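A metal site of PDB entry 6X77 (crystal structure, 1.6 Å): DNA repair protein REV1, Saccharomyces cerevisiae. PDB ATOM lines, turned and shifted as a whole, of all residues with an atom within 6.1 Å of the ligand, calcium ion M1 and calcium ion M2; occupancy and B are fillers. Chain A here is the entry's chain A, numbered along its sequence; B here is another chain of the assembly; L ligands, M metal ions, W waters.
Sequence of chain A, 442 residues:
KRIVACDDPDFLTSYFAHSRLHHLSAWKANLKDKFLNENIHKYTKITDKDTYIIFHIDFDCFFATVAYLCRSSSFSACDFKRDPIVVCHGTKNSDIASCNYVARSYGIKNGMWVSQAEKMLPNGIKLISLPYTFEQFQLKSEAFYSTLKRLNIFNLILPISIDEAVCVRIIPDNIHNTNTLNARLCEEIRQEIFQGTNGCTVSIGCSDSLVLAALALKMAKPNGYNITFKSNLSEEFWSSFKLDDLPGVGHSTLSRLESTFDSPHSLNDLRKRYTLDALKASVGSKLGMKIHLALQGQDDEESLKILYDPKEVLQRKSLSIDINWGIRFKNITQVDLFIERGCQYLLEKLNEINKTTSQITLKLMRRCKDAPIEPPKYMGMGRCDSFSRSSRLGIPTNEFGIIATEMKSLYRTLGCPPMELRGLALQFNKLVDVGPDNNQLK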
ATOM      1  N   ARG A  20     -32.911  15.508  -9.047  1.00  0.00           N
ATOM      2  CA  ARG A  20     -31.712  16.323  -8.835  1.00  0.00           C
ATOM      3  C   ARG A  20     -31.826  17.681  -9.529  1.00  0.00           C
ATOM      4  O   ARG A  20     -31.259  18.675  -9.028  1.00  0.00           O
ATOM      5  CB  ARG A  20     -30.475  15.546  -9.267  1.00  0.00           C
ATOM      6  CG  ARG A  20     -29.919  15.935 -10.615  1.00  0.00           C
ATOM      7  CD  ARG A  20     -30.565  15.190 -11.811  1.00  0.00           C
ATOM      8  NE  ARG A  20     -29.821  15.447 -13.041  1.00  0.00           N
ATOM      9  CZ  ARG A  20     -30.151  15.012 -14.253  1.00  0.00           C
ATOM     10  NH1 ARG A  20     -31.285  14.326 -14.480  1.00  0.00           N
ATOM     11  NH2 ARG A  20     -29.310  15.279 -15.267  1.00  0.00           N
ATOM     12  N   LEU A  21     -32.558  17.755 -10.639  1.00  0.00           N
ATOM     13  CA  LEU A  21     -32.731  19.049 -11.293  1.00  0.00           C
ATOM     14  C   LEU A  21     -33.568  19.986 -10.423  1.00  0.00           C
ATOM     15  O   LEU A  21     -33.245  21.176 -10.305  1.00  0.00           O
ATOM     16  CB  LEU A  21     -33.329  18.877 -12.686  1.00  0.00           C
ATOM     17  CG  LEU A  21     -32.384  18.115 -13.649  1.00  0.00           C
ATOM     18  CD1 LEU A  21     -33.027  17.867 -14.960  1.00  0.00           C
ATOM     19  CD2 LEU A  21     -31.048  18.800 -13.865  1.00  0.00           C
ATOM     20  N   LEU A  24     -31.065  21.157  -7.746  1.00  0.00           N
ATOM     21  CA  LEU A  24     -30.164  22.170  -8.293  1.00  0.00           C
ATOM     22  C   LEU A  24     -30.816  23.544  -8.306  1.00  0.00           C
ATOM     23  O   LEU A  24     -30.244  24.497  -7.807  1.00  0.00           O
ATOM     24  CB  LEU A  24     -29.727  21.806  -9.705  1.00  0.00           C
ATOM     25  CG  LEU A  24     -28.662  20.740  -9.773  1.00  0.00           C
ATOM     26  CD1 LEU A  24     -28.359  20.513 -11.277  1.00  0.00           C
ATOM     27  CD2 LEU A  24     -27.382  21.067  -9.067  1.00  0.00           C
ATOM     28  N   ASP A  58     -14.979  25.883  -8.668  1.00  0.00           N
ATOM     29  CA  ASP A  58     -16.018  24.881  -8.948  1.00  0.00           C
ATOM     30  C   ASP A  58     -15.555  23.486  -8.561  1.00  0.00           C
ATOM     31  O   ASP A  58     -14.425  23.090  -8.857  1.00  0.00           O
ATOM     32  CB  ASP A  58     -16.383  24.985 -10.436  1.00  0.00           C
ATOM     33  CG  ASP A  58     -17.211  23.813 -10.919  1.00  0.00           C
ATOM     34  OD1 ASP A  58     -18.453  23.902 -10.802  1.00  0.00           O
ATOM     35  OD2 ASP A  58     -16.593  22.807 -11.342  1.00  0.00           O
ATOM     36  N   PHE A  59     -16.438  22.741  -7.885  1.00  0.00           N
ATOM     37  CA  PHE A  59     -16.100  21.362  -7.518  1.00  0.00           C
ATOM     38  C   PHE A  59     -15.928  20.500  -8.775  1.00  0.00           C
ATOM     39  O   PHE A  59     -16.783  20.533  -9.667  1.00  0.00           O
ATOM     40  CB  PHE A  59     -17.223  20.695  -6.703  1.00  0.00           C
ATOM     41  CG  PHE A  59     -17.307  21.072  -5.266  1.00  0.00           C
ATOM     42  CD1 PHE A  59     -17.884  22.252  -4.889  1.00  0.00           C
ATOM     43  CD2 PHE A  59     -16.967  20.149  -4.305  1.00  0.00           C
ATOM     44  CE1 PHE A  59     -18.086  22.557  -3.519  1.00  0.00           C
ATOM     45  CE2 PHE A  59     -17.174  20.401  -2.939  1.00  0.00           C
ATOM     46  CZ  PHE A  59     -17.711  21.633  -2.563  1.00  0.00           C
ATOM     47  N   ASP A  60     -14.857  19.675  -8.805  1.00  0.00           N
ATOM     48  CA  ASP A  60     -14.715  18.651  -9.833  1.00  0.00           C
ATOM     49  C   ASP A  60     -15.675  17.463  -9.688  1.00  0.00           C
ATOM     50  O   ASP A  60     -15.762  16.824  -8.629  1.00  0.00           O
ATOM     51  CB  ASP A  60     -13.301  18.024  -9.776  1.00  0.00           C
ATOM     52  CG  ASP A  60     -12.226  19.072  -9.905  1.00  0.00           C
ATOM     53  OD1 ASP A  60     -12.315  19.921 -10.820  1.00  0.00           O
ATOM     54  OD2 ASP A  60     -11.318  19.040  -9.056  1.00  0.00           O
ATOM     55  N   CYS A  61     -16.396  17.164 -10.779  1.00  0.00           N
ATOM     56  CA  CYS A  61     -17.447  16.150 -10.848  1.00  0.00           C
ATOM     57  C   CYS A  61     -18.193  16.023  -9.519  1.00  0.00           C
ATOM     58  O   CYS A  61     -18.144  14.989  -8.838  1.00  0.00           O
ATOM     59  CB  CYS A  61     -16.875  14.808 -11.277  1.00  0.00           C
ATOM     60  SG  CYS A  61     -15.389  14.231 -10.334  1.00  0.00           S
ATOM     61  N   PHE A  62     -18.915  17.088  -9.169  1.00  0.00           N
ATOM     62  CA  PHE A  62     -19.385  17.291  -7.800  1.00  0.00           C
ATOM     63  C   PHE A  62     -20.161  16.110  -7.227  1.00  0.00           C
ATOM     64  O   PHE A  62     -19.800  15.590  -6.172  1.00  0.00           O
ATOM     65  CB  PHE A  62     -20.220  18.574  -7.762  1.00  0.00           C
ATOM     66  CG  PHE A  62     -20.793  18.917  -6.413  1.00  0.00           C
ATOM     67  CD1 PHE A  62     -19.979  19.046  -5.301  1.00  0.00           C
ATOM     68  CD2 PHE A  62     -22.158  19.173  -6.274  1.00  0.00           C
ATOM     69  CE1 PHE A  62     -20.504  19.386  -4.074  1.00  0.00           C
ATOM     70  CE2 PHE A  62     -22.692  19.557  -5.037  1.00  0.00           C
ATOM     71  CZ  PHE A  62     -21.878  19.632  -3.938  1.00  0.00           C
ATOM     72  N   PHE A  63     -21.289  15.747  -7.851  1.00  0.00           N
ATOM     73  CA  PHE A  63     -22.086  14.672  -7.252  1.00  0.00           C
ATOM     74  C   PHE A  63     -21.259  13.389  -7.181  1.00  0.00           C
ATOM     75  O   PHE A  63     -21.379  12.641  -6.219  1.00  0.00           O
ATOM     76  CB  PHE A  63     -23.372  14.344  -8.017  1.00  0.00           C
ATOM     77  CG  PHE A  63     -24.499  15.336  -7.853  1.00  0.00           C
ATOM     78  CD1 PHE A  63     -24.330  16.537  -7.181  1.00  0.00           C
ATOM     79  CD2 PHE A  63     -25.755  15.042  -8.384  1.00  0.00           C
ATOM     80  CE1 PHE A  63     -25.347  17.453  -7.095  1.00  0.00           C
ATOM     81  CE2 PHE A  63     -26.798  15.960  -8.289  1.00  0.00           C
ATOM     82  CZ  PHE A  63     -26.598  17.147  -7.633  1.00  0.00           C
ATOM     83  N   ALA A  64     -20.486  13.089  -8.236  1.00  0.00           N
ATOM     84  CA  ALA A  64     -19.690  11.852  -8.246  1.00  0.00           C
ATOM     85  C   ALA A  64     -18.698  11.856  -7.091  1.00  0.00           C
ATOM     86  O   ALA A  64     -18.620  10.876  -6.338  1.00  0.00           O
ATOM     87  CB  ALA A  64     -19.005  11.660  -9.602  1.00  0.00           C
ATOM     88  N   ASP A  95     -30.583   9.370 -16.306  1.00  0.00           N
ATOM     89  CA  ASP A  95     -29.530  10.361 -16.470  1.00  0.00           C
ATOM     90  C   ASP A  95     -28.332  10.085 -15.556  1.00  0.00           C
ATOM     91  O   ASP A  95     -28.469   9.817 -14.364  1.00  0.00           O
ATOM     92  CB  ASP A  95     -30.045  11.767 -16.194  1.00  0.00           C
ATOM     93  CG  ASP A  95     -30.796  12.380 -17.357  1.00  0.00           C
ATOM     94  OD1 ASP A  95     -31.258  11.692 -18.293  1.00  0.00           O
ATOM     95  OD2 ASP A  95     -30.974  13.604 -17.289  1.00  0.00           O
ATOM     96  N   ILE A  96     -27.153  10.196 -16.137  1.00  0.00           N
ATOM     97  CA  ILE A  96     -25.909  10.356 -15.396  1.00  0.00           C
ATOM     98  C   ILE A  96     -25.831  11.820 -14.952  1.00  0.00           C
ATOM     99  O   ILE A  96     -25.479  12.723 -15.728  1.00  0.00           O
ATOM    100  CB  ILE A  96     -24.701   9.938 -16.248  1.00  0.00           C
ATOM    101  CG1 ILE A  96     -24.759   8.420 -16.491  1.00  0.00           C
ATOM    102  CG2 ILE A  96     -23.433  10.335 -15.550  1.00  0.00           C
ATOM    103  CD1 ILE A  96     -23.918   7.977 -17.712  1.00  0.00           C
ATOM    104  N   ALA A  97     -26.150  12.067 -13.675  1.00  0.00           N
ATOM    105  CA  ALA A  97     -26.089  13.434 -13.154  1.00  0.00           C
ATOM    106  C   ALA A  97     -24.663  13.948 -13.135  1.00  0.00           C
ATOM    107  O   ALA A  97     -24.438  15.128 -13.459  1.00  0.00           O
ATOM    108  CB  ALA A  97     -26.712  13.523 -11.748  1.00  0.00           C
ATOM    109  N   SER A  98     -23.694  13.087 -12.757  1.00  0.00           N
ATOM    110  CA  SER A  98     -22.269  13.409 -12.679  1.00  0.00           C
ATOM    111  C   SER A  98     -21.471  12.131 -12.918  1.00  0.00           C
ATOM    112  O   SER A  98     -21.891  11.044 -12.481  1.00  0.00           O
ATOM    113  CB  SER A  98     -21.887  14.051 -11.333  1.00  0.00           C
ATOM    114  OG  SER A  98     -20.532  14.513 -11.272  1.00  0.00           O
ATOM    115  N   CYS A  99     -20.337  12.274 -13.595  1.00  0.00           N
ATOM    116  CA  CYS A  99     -19.395  11.181 -13.820  1.00  0.00           C
ATOM    117  C   CYS A  99     -17.993  11.667 -13.513  1.00  0.00           C
ATOM    118  O   CYS A  99     -17.664  12.863 -13.687  1.00  0.00           O
ATOM    119  CB  CYS A  99     -19.510  10.642 -15.256  1.00  0.00           C
ATOM    120  SG  CYS A  99     -19.229  11.877 -16.547  1.00  0.00           S
ATOM    121  N   TYR A 101     -13.662  11.539 -13.694  1.00  0.00           N
ATOM    122  CA  TYR A 101     -12.855  11.802 -14.894  1.00  0.00           C
ATOM    123  C   TYR A 101     -12.353  10.515 -15.514  1.00  0.00           C
ATOM    124  O   TYR A 101     -12.130  10.505 -16.725  1.00  0.00           O
ATOM    125  CB  TYR A 101     -11.726  12.791 -14.568  1.00  0.00           C
ATOM    126  CG  TYR A 101     -12.275  14.197 -14.569  1.00  0.00           C
ATOM    127  CD1 TYR A 101     -13.155  14.640 -13.571  1.00  0.00           C
ATOM    128  CD2 TYR A 101     -11.980  15.074 -15.594  1.00  0.00           C
ATOM    129  CE1 TYR A 101     -13.700  15.914 -13.626  1.00  0.00           C
ATOM    130  CE2 TYR A 101     -12.508  16.340 -15.638  1.00  0.00           C
ATOM    131  CZ  TYR A 101     -13.366  16.769 -14.660  1.00  0.00           C
ATOM    132  OH  TYR A 101     -13.867  18.052 -14.718  1.00  0.00           O
ATOM    133  N   ARG A 104     -15.050   9.903 -17.928  1.00  0.00           N
ATOM    134  CA  ARG A 104     -14.966  10.847 -19.035  1.00  0.00           C
ATOM    135  C   ARG A 104     -13.839  10.519 -20.012  1.00  0.00           C
ATOM    136  O   ARG A 104     -13.898  10.946 -21.172  1.00  0.00           O
ATOM    137  CB  ARG A 104     -14.771  12.256 -18.501  1.00  0.00           C
ATOM    138  CG  ARG A 104     -15.952  12.721 -17.667  1.00  0.00           C
ATOM    139  CD  ARG A 104     -15.779  14.156 -17.160  1.00  0.00           C
ATOM    140  NE  ARG A 104     -16.763  14.417 -16.099  1.00  0.00           N
ATOM    141  CZ  ARG A 104     -17.075  15.614 -15.629  1.00  0.00           C
ATOM    142  NH1 ARG A 104     -16.500  16.711 -16.116  1.00  0.00           N
ATOM    143  NH2 ARG A 104     -17.998  15.695 -14.664  1.00  0.00           N
ATOM    144  N   ASN A 110     -21.746  14.105 -18.385  1.00  0.00           N
ATOM    145  CA  ASN A 110     -22.956  14.418 -17.604  1.00  0.00           C
ATOM    146  C   ASN A 110     -24.146  14.578 -18.537  1.00  0.00           C
ATOM    147  O   ASN A 110     -24.033  15.171 -19.621  1.00  0.00           O
ATOM    148  CB  ASN A 110     -22.777  15.712 -16.808  1.00  0.00           C
ATOM    149  CG  ASN A 110     -21.759  15.589 -15.683  1.00  0.00           C
ATOM    150  OD1 ASN A 110     -21.222  14.517 -15.411  1.00  0.00           O
ATOM    151  ND2 ASN A 110     -21.474  16.714 -15.030  1.00  0.00           N
ATOM    152  N   GLY A 111     -25.282  14.028 -18.135  1.00  0.00           N
ATOM    153  CA  GLY A 111     -26.507  14.085 -18.908  1.00  0.00           C
ATOM    154  C   GLY A 111     -26.745  12.894 -19.809  1.00  0.00           C
ATOM    155  O   GLY A 111     -27.883  12.686 -20.252  1.00  0.00           O
ATOM    156  N   TYR A 132     -27.663   8.941  -5.404  1.00  0.00           N
ATOM    157  CA  TYR A 132     -27.603  10.305  -4.951  1.00  0.00           C
ATOM    158  C   TYR A 132     -27.492  10.371  -3.428  1.00  0.00           C
ATOM    159  O   TYR A 132     -28.102   9.581  -2.711  1.00  0.00           O
ATOM    160  CB  TYR A 132     -28.855  11.045  -5.390  1.00  0.00           C
ATOM    161  CG  TYR A 132     -29.036  11.205  -6.899  1.00  0.00           C
ATOM    162  CD1 TYR A 132     -29.732  10.276  -7.656  1.00  0.00           C
ATOM    163  CD2 TYR A 132     -28.526  12.312  -7.555  1.00  0.00           C
ATOM    164  CE1 TYR A 132     -29.942  10.464  -9.016  1.00  0.00           C
ATOM    165  CE2 TYR A 132     -28.679  12.465  -8.937  1.00  0.00           C
ATOM    166  CZ  TYR A 132     -29.409  11.565  -9.649  1.00  0.00           C
ATOM    167  OH  TYR A 132     -29.646  11.735 -10.996  1.00  0.00           O
ATOM    168  N   SER A 161     -23.882  28.179  -8.387  1.00  0.00           N
ATOM    169  CA  SER A 161     -24.688  26.992  -8.122  1.00  0.00           C
ATOM    170  C   SER A 161     -24.159  26.351  -6.838  1.00  0.00           C
ATOM    171  O   SER A 161     -23.267  26.876  -6.168  1.00  0.00           O
ATOM    172  CB  SER A 161     -24.646  26.022  -9.299  1.00  0.00           C
ATOM    173  OG  SER A 161     -23.385  25.366  -9.290  1.00  0.00           O
ATOM    174  N   ILE A 162     -24.794  25.241  -6.480  1.00  0.00           N
ATOM    175  CA  ILE A 162     -24.461  24.446  -5.319  1.00  0.00           C
ATOM    176  C   ILE A 162     -22.941  24.250  -5.234  1.00  0.00           C
ATOM    177  O   ILE A 162     -22.378  24.286  -4.138  1.00  0.00           O
ATOM    178  CB  ILE A 162     -25.205  23.095  -5.388  1.00  0.00           C
ATOM    179  CG1 ILE A 162     -25.008  22.331  -4.064  1.00  0.00           C
ATOM    180  CG2 ILE A 162     -24.858  22.266  -6.623  1.00  0.00           C
ATOM    181  CD1 ILE A 162     -25.698  22.965  -2.962  1.00  0.00           C
ATOM    182  N   ASP A 163     -22.261  24.058  -6.367  1.00  0.00           N
ATOM    183  CA  ASP A 163     -20.841  23.712  -6.326  1.00  0.00           C
ATOM    184  C   ASP A 163     -19.933  24.745  -6.987  1.00  0.00           C
ATOM    185  O   ASP A 163     -18.786  24.401  -7.329  1.00  0.00           O
ATOM    186  CB  ASP A 163     -20.617  22.341  -6.977  1.00  0.00           C
ATOM    187  CG  ASP A 163     -20.567  22.423  -8.516  1.00  0.00           C
ATOM    188  OD1 ASP A 163     -21.301  23.259  -9.079  1.00  0.00           O
ATOM    189  OD2 ASP A 163     -19.815  21.627  -9.116  1.00  0.00           O
ATOM    190  N   GLU A 164     -20.373  25.994  -7.120  1.00  0.00           N
ATOM    191  CA  GLU A 164     -19.656  26.904  -8.010  1.00  0.00           C
ATOM    192  C   GLU A 164     -19.891  28.348  -7.627  1.00  0.00           C
ATOM    193  O   GLU A 164     -21.039  28.754  -7.388  1.00  0.00           O
ATOM    194  CB  GLU A 164     -20.094  26.662  -9.447  1.00  0.00           C
ATOM    195  CG  GLU A 164     -19.398  27.440 -10.504  1.00  0.00           C
ATOM    196  CD  GLU A 164     -19.851  27.041 -11.908  1.00  0.00           C
ATOM    197  OE1 GLU A 164     -19.440  27.757 -12.868  1.00  0.00           O
ATOM    198  OE2 GLU A 164     -20.660  26.055 -12.043  1.00  0.00           O
ATOM    199  N   LYS A 218     -12.129  25.549 -17.138  1.00  0.00           N
ATOM    200  CA  LYS A 218     -12.193  24.366 -17.988  1.00  0.00           C
ATOM    201  C   LYS A 218     -10.804  23.784 -18.235  1.00  0.00           C
ATOM    202  O   LYS A 218     -10.583  22.589 -18.095  1.00  0.00           O
ATOM    203  CB  LYS A 218     -12.849  24.737 -19.307  1.00  0.00           C
ATOM    204  CG  LYS A 218     -13.238  23.557 -20.150  1.00  0.00           C
ATOM    205  CD  LYS A 218     -14.448  22.964 -19.539  1.00  0.00           C
ATOM    206  CE  LYS A 218     -14.392  21.455 -19.557  1.00  0.00           C
ATOM    207  NZ  LYS A 218     -13.604  20.873 -20.711  1.00  0.00           N
ATOM    208  N   LYS A 221      -9.223  21.815 -15.132  1.00  0.00           N
ATOM    209  CA  LYS A 221      -9.786  20.566 -14.645  1.00  0.00           C
ATOM    210  C   LYS A 221      -9.077  19.338 -15.219  1.00  0.00           C
ATOM    211  O   LYS A 221      -8.593  19.370 -16.354  1.00  0.00           O
ATOM    212  CB  LYS A 221     -11.262  20.520 -14.991  1.00  0.00           C
ATOM    213  CG  LYS A 221     -12.117  21.460 -14.107  1.00  0.00           C
ATOM    214  CD  LYS A 221     -13.579  21.463 -14.466  1.00  0.00           C
ATOM    215  CE  LYS A 221     -14.362  22.252 -13.406  1.00  0.00           C
ATOM    216  NZ  LYS A 221     -14.492  21.460 -12.135  1.00  0.00           N
ATOM    217  P    DG B  12     -24.233  28.391 -15.089  1.00  0.00           P
ATOM    218  OP1  DG B  12     -24.774  29.624 -14.704  1.00  0.00           O
ATOM    219  OP2  DG B  12     -22.966  28.337 -15.731  1.00  0.00           O
ATOM    220  O5'  DG B  12     -24.238  27.517 -13.763  1.00  0.00           O
ATOM    221  C5'  DG B  12     -23.566  26.274 -13.698  1.00  0.00           C
ATOM    222  C4'  DG B  12     -24.489  25.203 -13.139  1.00  0.00           C
ATOM    223  O4'  DG B  12     -25.499  24.925 -14.071  1.00  0.00           O
ATOM    224  C3'  DG B  12     -23.790  23.875 -12.931  1.00  0.00           C
ATOM    225  O3'  DG B  12     -23.275  23.798 -11.622  1.00  0.00           O
ATOM    226  C2'  DG B  12     -24.887  22.859 -13.180  1.00  0.00           C
ATOM    227  C1'  DG B  12     -26.050  23.688 -13.682  1.00  0.00           C
ATOM    228  N9   DG B  12     -26.795  23.141 -14.795  1.00  0.00           N
ATOM    229  C8   DG B  12     -26.343  22.541 -15.941  1.00  0.00           C
ATOM    230  N7   DG B  12     -27.312  22.177 -16.735  1.00  0.00           N
ATOM    231  C5   DG B  12     -28.465  22.531 -16.058  1.00  0.00           C
ATOM    232  C6   DG B  12     -29.829  22.388 -16.433  1.00  0.00           C
ATOM    233  O6   DG B  12     -30.296  21.845 -17.409  1.00  0.00           O
ATOM    234  N1   DG B  12     -30.673  22.899 -15.452  1.00  0.00           N
ATOM    235  C2   DG B  12     -30.267  23.487 -14.287  1.00  0.00           C
ATOM    236  N2   DG B  12     -31.239  23.868 -13.458  1.00  0.00           N
ATOM    237  N3   DG B  12     -29.005  23.618 -13.927  1.00  0.00           N
ATOM    238  C4   DG B  12     -28.165  23.117 -14.855  1.00  0.00           C
HETATM  239  N1  LIG L   1     -25.733  18.203 -12.863  1.00  0.00           N
HETATM  240  C1  LIG L   1     -26.782  17.230 -13.266  1.00  0.00           C
HETATM  241  N2  LIG L   1     -27.050  17.059 -14.700  1.00  0.00           N
HETATM  242  C2  LIG L   1     -26.255  17.731 -15.666  1.00  0.00           C
HETATM  243  C3  LIG L   1     -25.179  18.663 -15.265  1.00  0.00           C
HETATM  244  C4  LIG L   1     -24.915  18.885 -13.831  1.00  0.00           C
HETATM  245  O1  LIG L   1     -27.458  16.630 -12.515  1.00  0.00           O
HETATM  246  N3  LIG L   1     -26.478  17.499 -17.044  1.00  0.00           N
HETATM  247  C5  LIG L   1     -25.420  18.404 -11.435  1.00  0.00           C
HETATM  248  C6  LIG L   1     -24.423  17.228 -11.108  1.00  0.00           C
HETATM  249  C7  LIG L   1     -23.068  17.886 -11.196  1.00  0.00           C
HETATM  250  C8  LIG L   1     -23.330  19.091 -10.624  1.00  0.00           C
HETATM  251  O2  LIG L   1     -24.770  19.498 -11.217  1.00  0.00           O
HETATM  252  O3  LIG L   1     -22.101  17.267 -10.276  1.00  0.00           O
HETATM  253  C9  LIG L   1     -22.546  20.314 -10.918  1.00  0.00           C
HETATM  254  O4  LIG L   1     -22.619  20.534 -12.317  1.00  0.00           O
HETATM  255  P1  LIG L   1     -21.261  20.867 -13.123  1.00  0.00           P
HETATM  256  O5  LIG L   1     -20.427  21.887 -12.416  1.00  0.00           O
HETATM  257  O6  LIG L   1     -21.654  21.280 -14.536  1.00  0.00           O
HETATM  258  O7  LIG L   1     -20.514  19.458 -13.351  1.00  0.00           O
HETATM  259  P2  LIG L   1     -19.644  18.448 -12.462  1.00  0.00           P
HETATM  260  O8  LIG L   1     -19.271  19.131 -11.173  1.00  0.00           O
HETATM  261  O9  LIG L   1     -20.318  17.098 -12.305  1.00  0.00           O
HETATM  262  O10 LIG L   1     -18.340  18.234 -13.362  1.00  0.00           O
HETATM  263  P3  LIG L   1     -17.178  19.332 -13.774  1.00  0.00           P
HETATM  264  O11 LIG L   1     -17.547  20.684 -13.236  1.00  0.00           O
HETATM  265  O12 LIG L   1     -15.896  18.871 -13.146  1.00  0.00           O
HETATM  266  O13 LIG L   1     -17.129  19.277 -15.288  1.00  0.00           O
HETATM  267 CA    CA M   1     -18.511  21.315 -11.048  1.00  0.00          CA
HETATM  268 CA    CA M   2     -20.871  23.760 -11.368  1.00  0.00          CA
HETATM  269  O   HOH W   1     -16.044  21.084 -17.035  1.00  0.00           O
HETATM  270  O   HOH W   2     -22.026  19.176 -16.418  1.00  0.00           O
HETATM  271  O   HOH W   3     -25.164  19.124 -19.006  1.00  0.00           O
HETATM  272  O   HOH W   4     -29.016  16.473 -18.160  1.00  0.00           O
HETATM  273  O   HOH W   5     -22.808  23.301 -16.239  1.00  0.00           O
HETATM  274  O   HOH W   6     -19.238  18.868 -16.851  1.00  0.00           O
HETATM  275  O   HOH W   7     -17.854  23.149 -14.764  1.00  0.00           O
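Calcium ion M1 is bound by an oxygen (O8) of the ligand, at 2.3 Å.
The backbone carbonyl oxygen (O) of Phe 59 binds calcium ion M1 (2.3 Å).
Calcium ion M1 is bound by OD2 of Asp 163, 2.4 Å away.
An oxygen (O5) of the ligand binds calcium ion M1, 2.4 Å away.
OD2 of Asp 58 is bound to calcium ion M1 (2.4 Å).
O11 of the ligand is bound to calcium ion M1, 2.5 Å away.
OD1 of Asp 58 is bound to calcium ion M1 (2.6 Å).
Calcium ion M1 has seven donor atoms within binding distance.
The backbone carbonyl oxygen (O) of Ala 97 sits close to a nitrogen (N1) of the ligand, at 3.4 Å.
CD1 of Leu 24 touches C5 of the ligand, 3.6 Å away.
CA of Asp 60 touches O12 of the ligand, 3.5 Å away.
Gly 111 touches the ligand (N to N3, 3.8 Å).
Hydrophobic or aromatic side chains within 4 Å of the ligand: Leu 24, Phe 62, Phe 63, Ala 97 and Tyr 101.
Within 4 Å of the ligand: Arg 20, Leu 24, Asp 58, Phe 59, Asp 60, Cys 61, Phe 62, Phe 63, Ala 97, Ser 98, Tyr 101, Arg 104, Asn 110, Gly 111, Asp 163, Lys 221 and DG 12 of chain B.
Water W2 lies within hydrogen-bond range of O6 of the ligand and ND2 of Asn 110.
Water W4 bridges a nitrogen (N3) of the ligand and the guanidinium group (NH2) of Arg 20.
The side-chain hydroxyl (OG) of Ser 161 lies close to the backbone NH (N) of Asp 163, at 3.4 Å.
The side-chain hydroxyl (OH) of Tyr 101 sits at hydrogen-bond distance from the guanidinium group (NH1) of Arg 104.
The side-chain hydroxyl of Ser 98 lies within hydrogen-bond range of the backbone NH of Ala 64, 3.4 Å away.
O of Cys 99 lies within hydrogen-bond range of NE of Arg 104, at 3.0 Å.
The backbone NH of Gly 111 is in hydrogen-bond range of the backbone carbonyl oxygen of Ile 96.
The backbone carbonyl oxygen of Cys 61 sits close to the side-chain hydroxyl of Ser 98 (3.4 Å).
O3' of DG 12 of chain B sits close to the side-chain hydroxyl of Ser 161, 2.8 Å away.
O of Phe 59 sits close to NZ of Lys 221, at 3.5 Å.
An oxygen (O5) of the ligand is bound to calcium ion M2.
The side-chain carboxylate (OD1) of Asp 163 binds calcium ion M2 (2.4 Å).
Calcium ion M2 is bound by the side-chain carboxylate (OE2) of Glu 164 (2.4 Å).
Calcium ion M2 is bound by O3' of DG 12 of chain B (2.4 Å).
The side-chain carboxylate (OD1) of Asp 58 is bound to calcium ion M2, 2.5 Å away.
An oxygen (O9) of the ligand is in hydrogen-bond range of the side-chain hydroxyl (OG) of Ser 98 (2.8 Å).
N of Cys 61 lies within hydrogen-bond range of O12 of the ligand (3.0 Å).
The side-chain hydroxyl (OH) of Tyr 101 lies within hydrogen-bond range of an oxygen (O12) of the ligand (2.7 Å).
O13 of the ligand lies within salt-bridge range of NH1 of Arg 104.
N of Phe 63 sits at hydrogen-bond distance from O3 of the ligand.
NE of Arg 20 is in hydrogen-bond range of O1 of the ligand, 2.7 Å away.
The backbone NH of Phe 62 is in hydrogen-bond range of an oxygen (O3) of the ligand, at 3.4 Å.
An oxygen (O12) of the ligand is in salt-bridge range of the side-chain amino group of Lys 221, 3.1 Å away.
An oxygen (O9) of the ligand sits at hydrogen-bond distance from the side-chain amide nitrogen (ND2) of Asn 110 (3.0 Å).
OG of Ser 161 touches calcium ion M2 (3.6 Å).
Along chain A the residues within 4 Å of calcium ion M1 span positions 58 to 163.
The nearest printed residue that does not touch calcium ion M1 is Lys 221 (4.2 Å).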
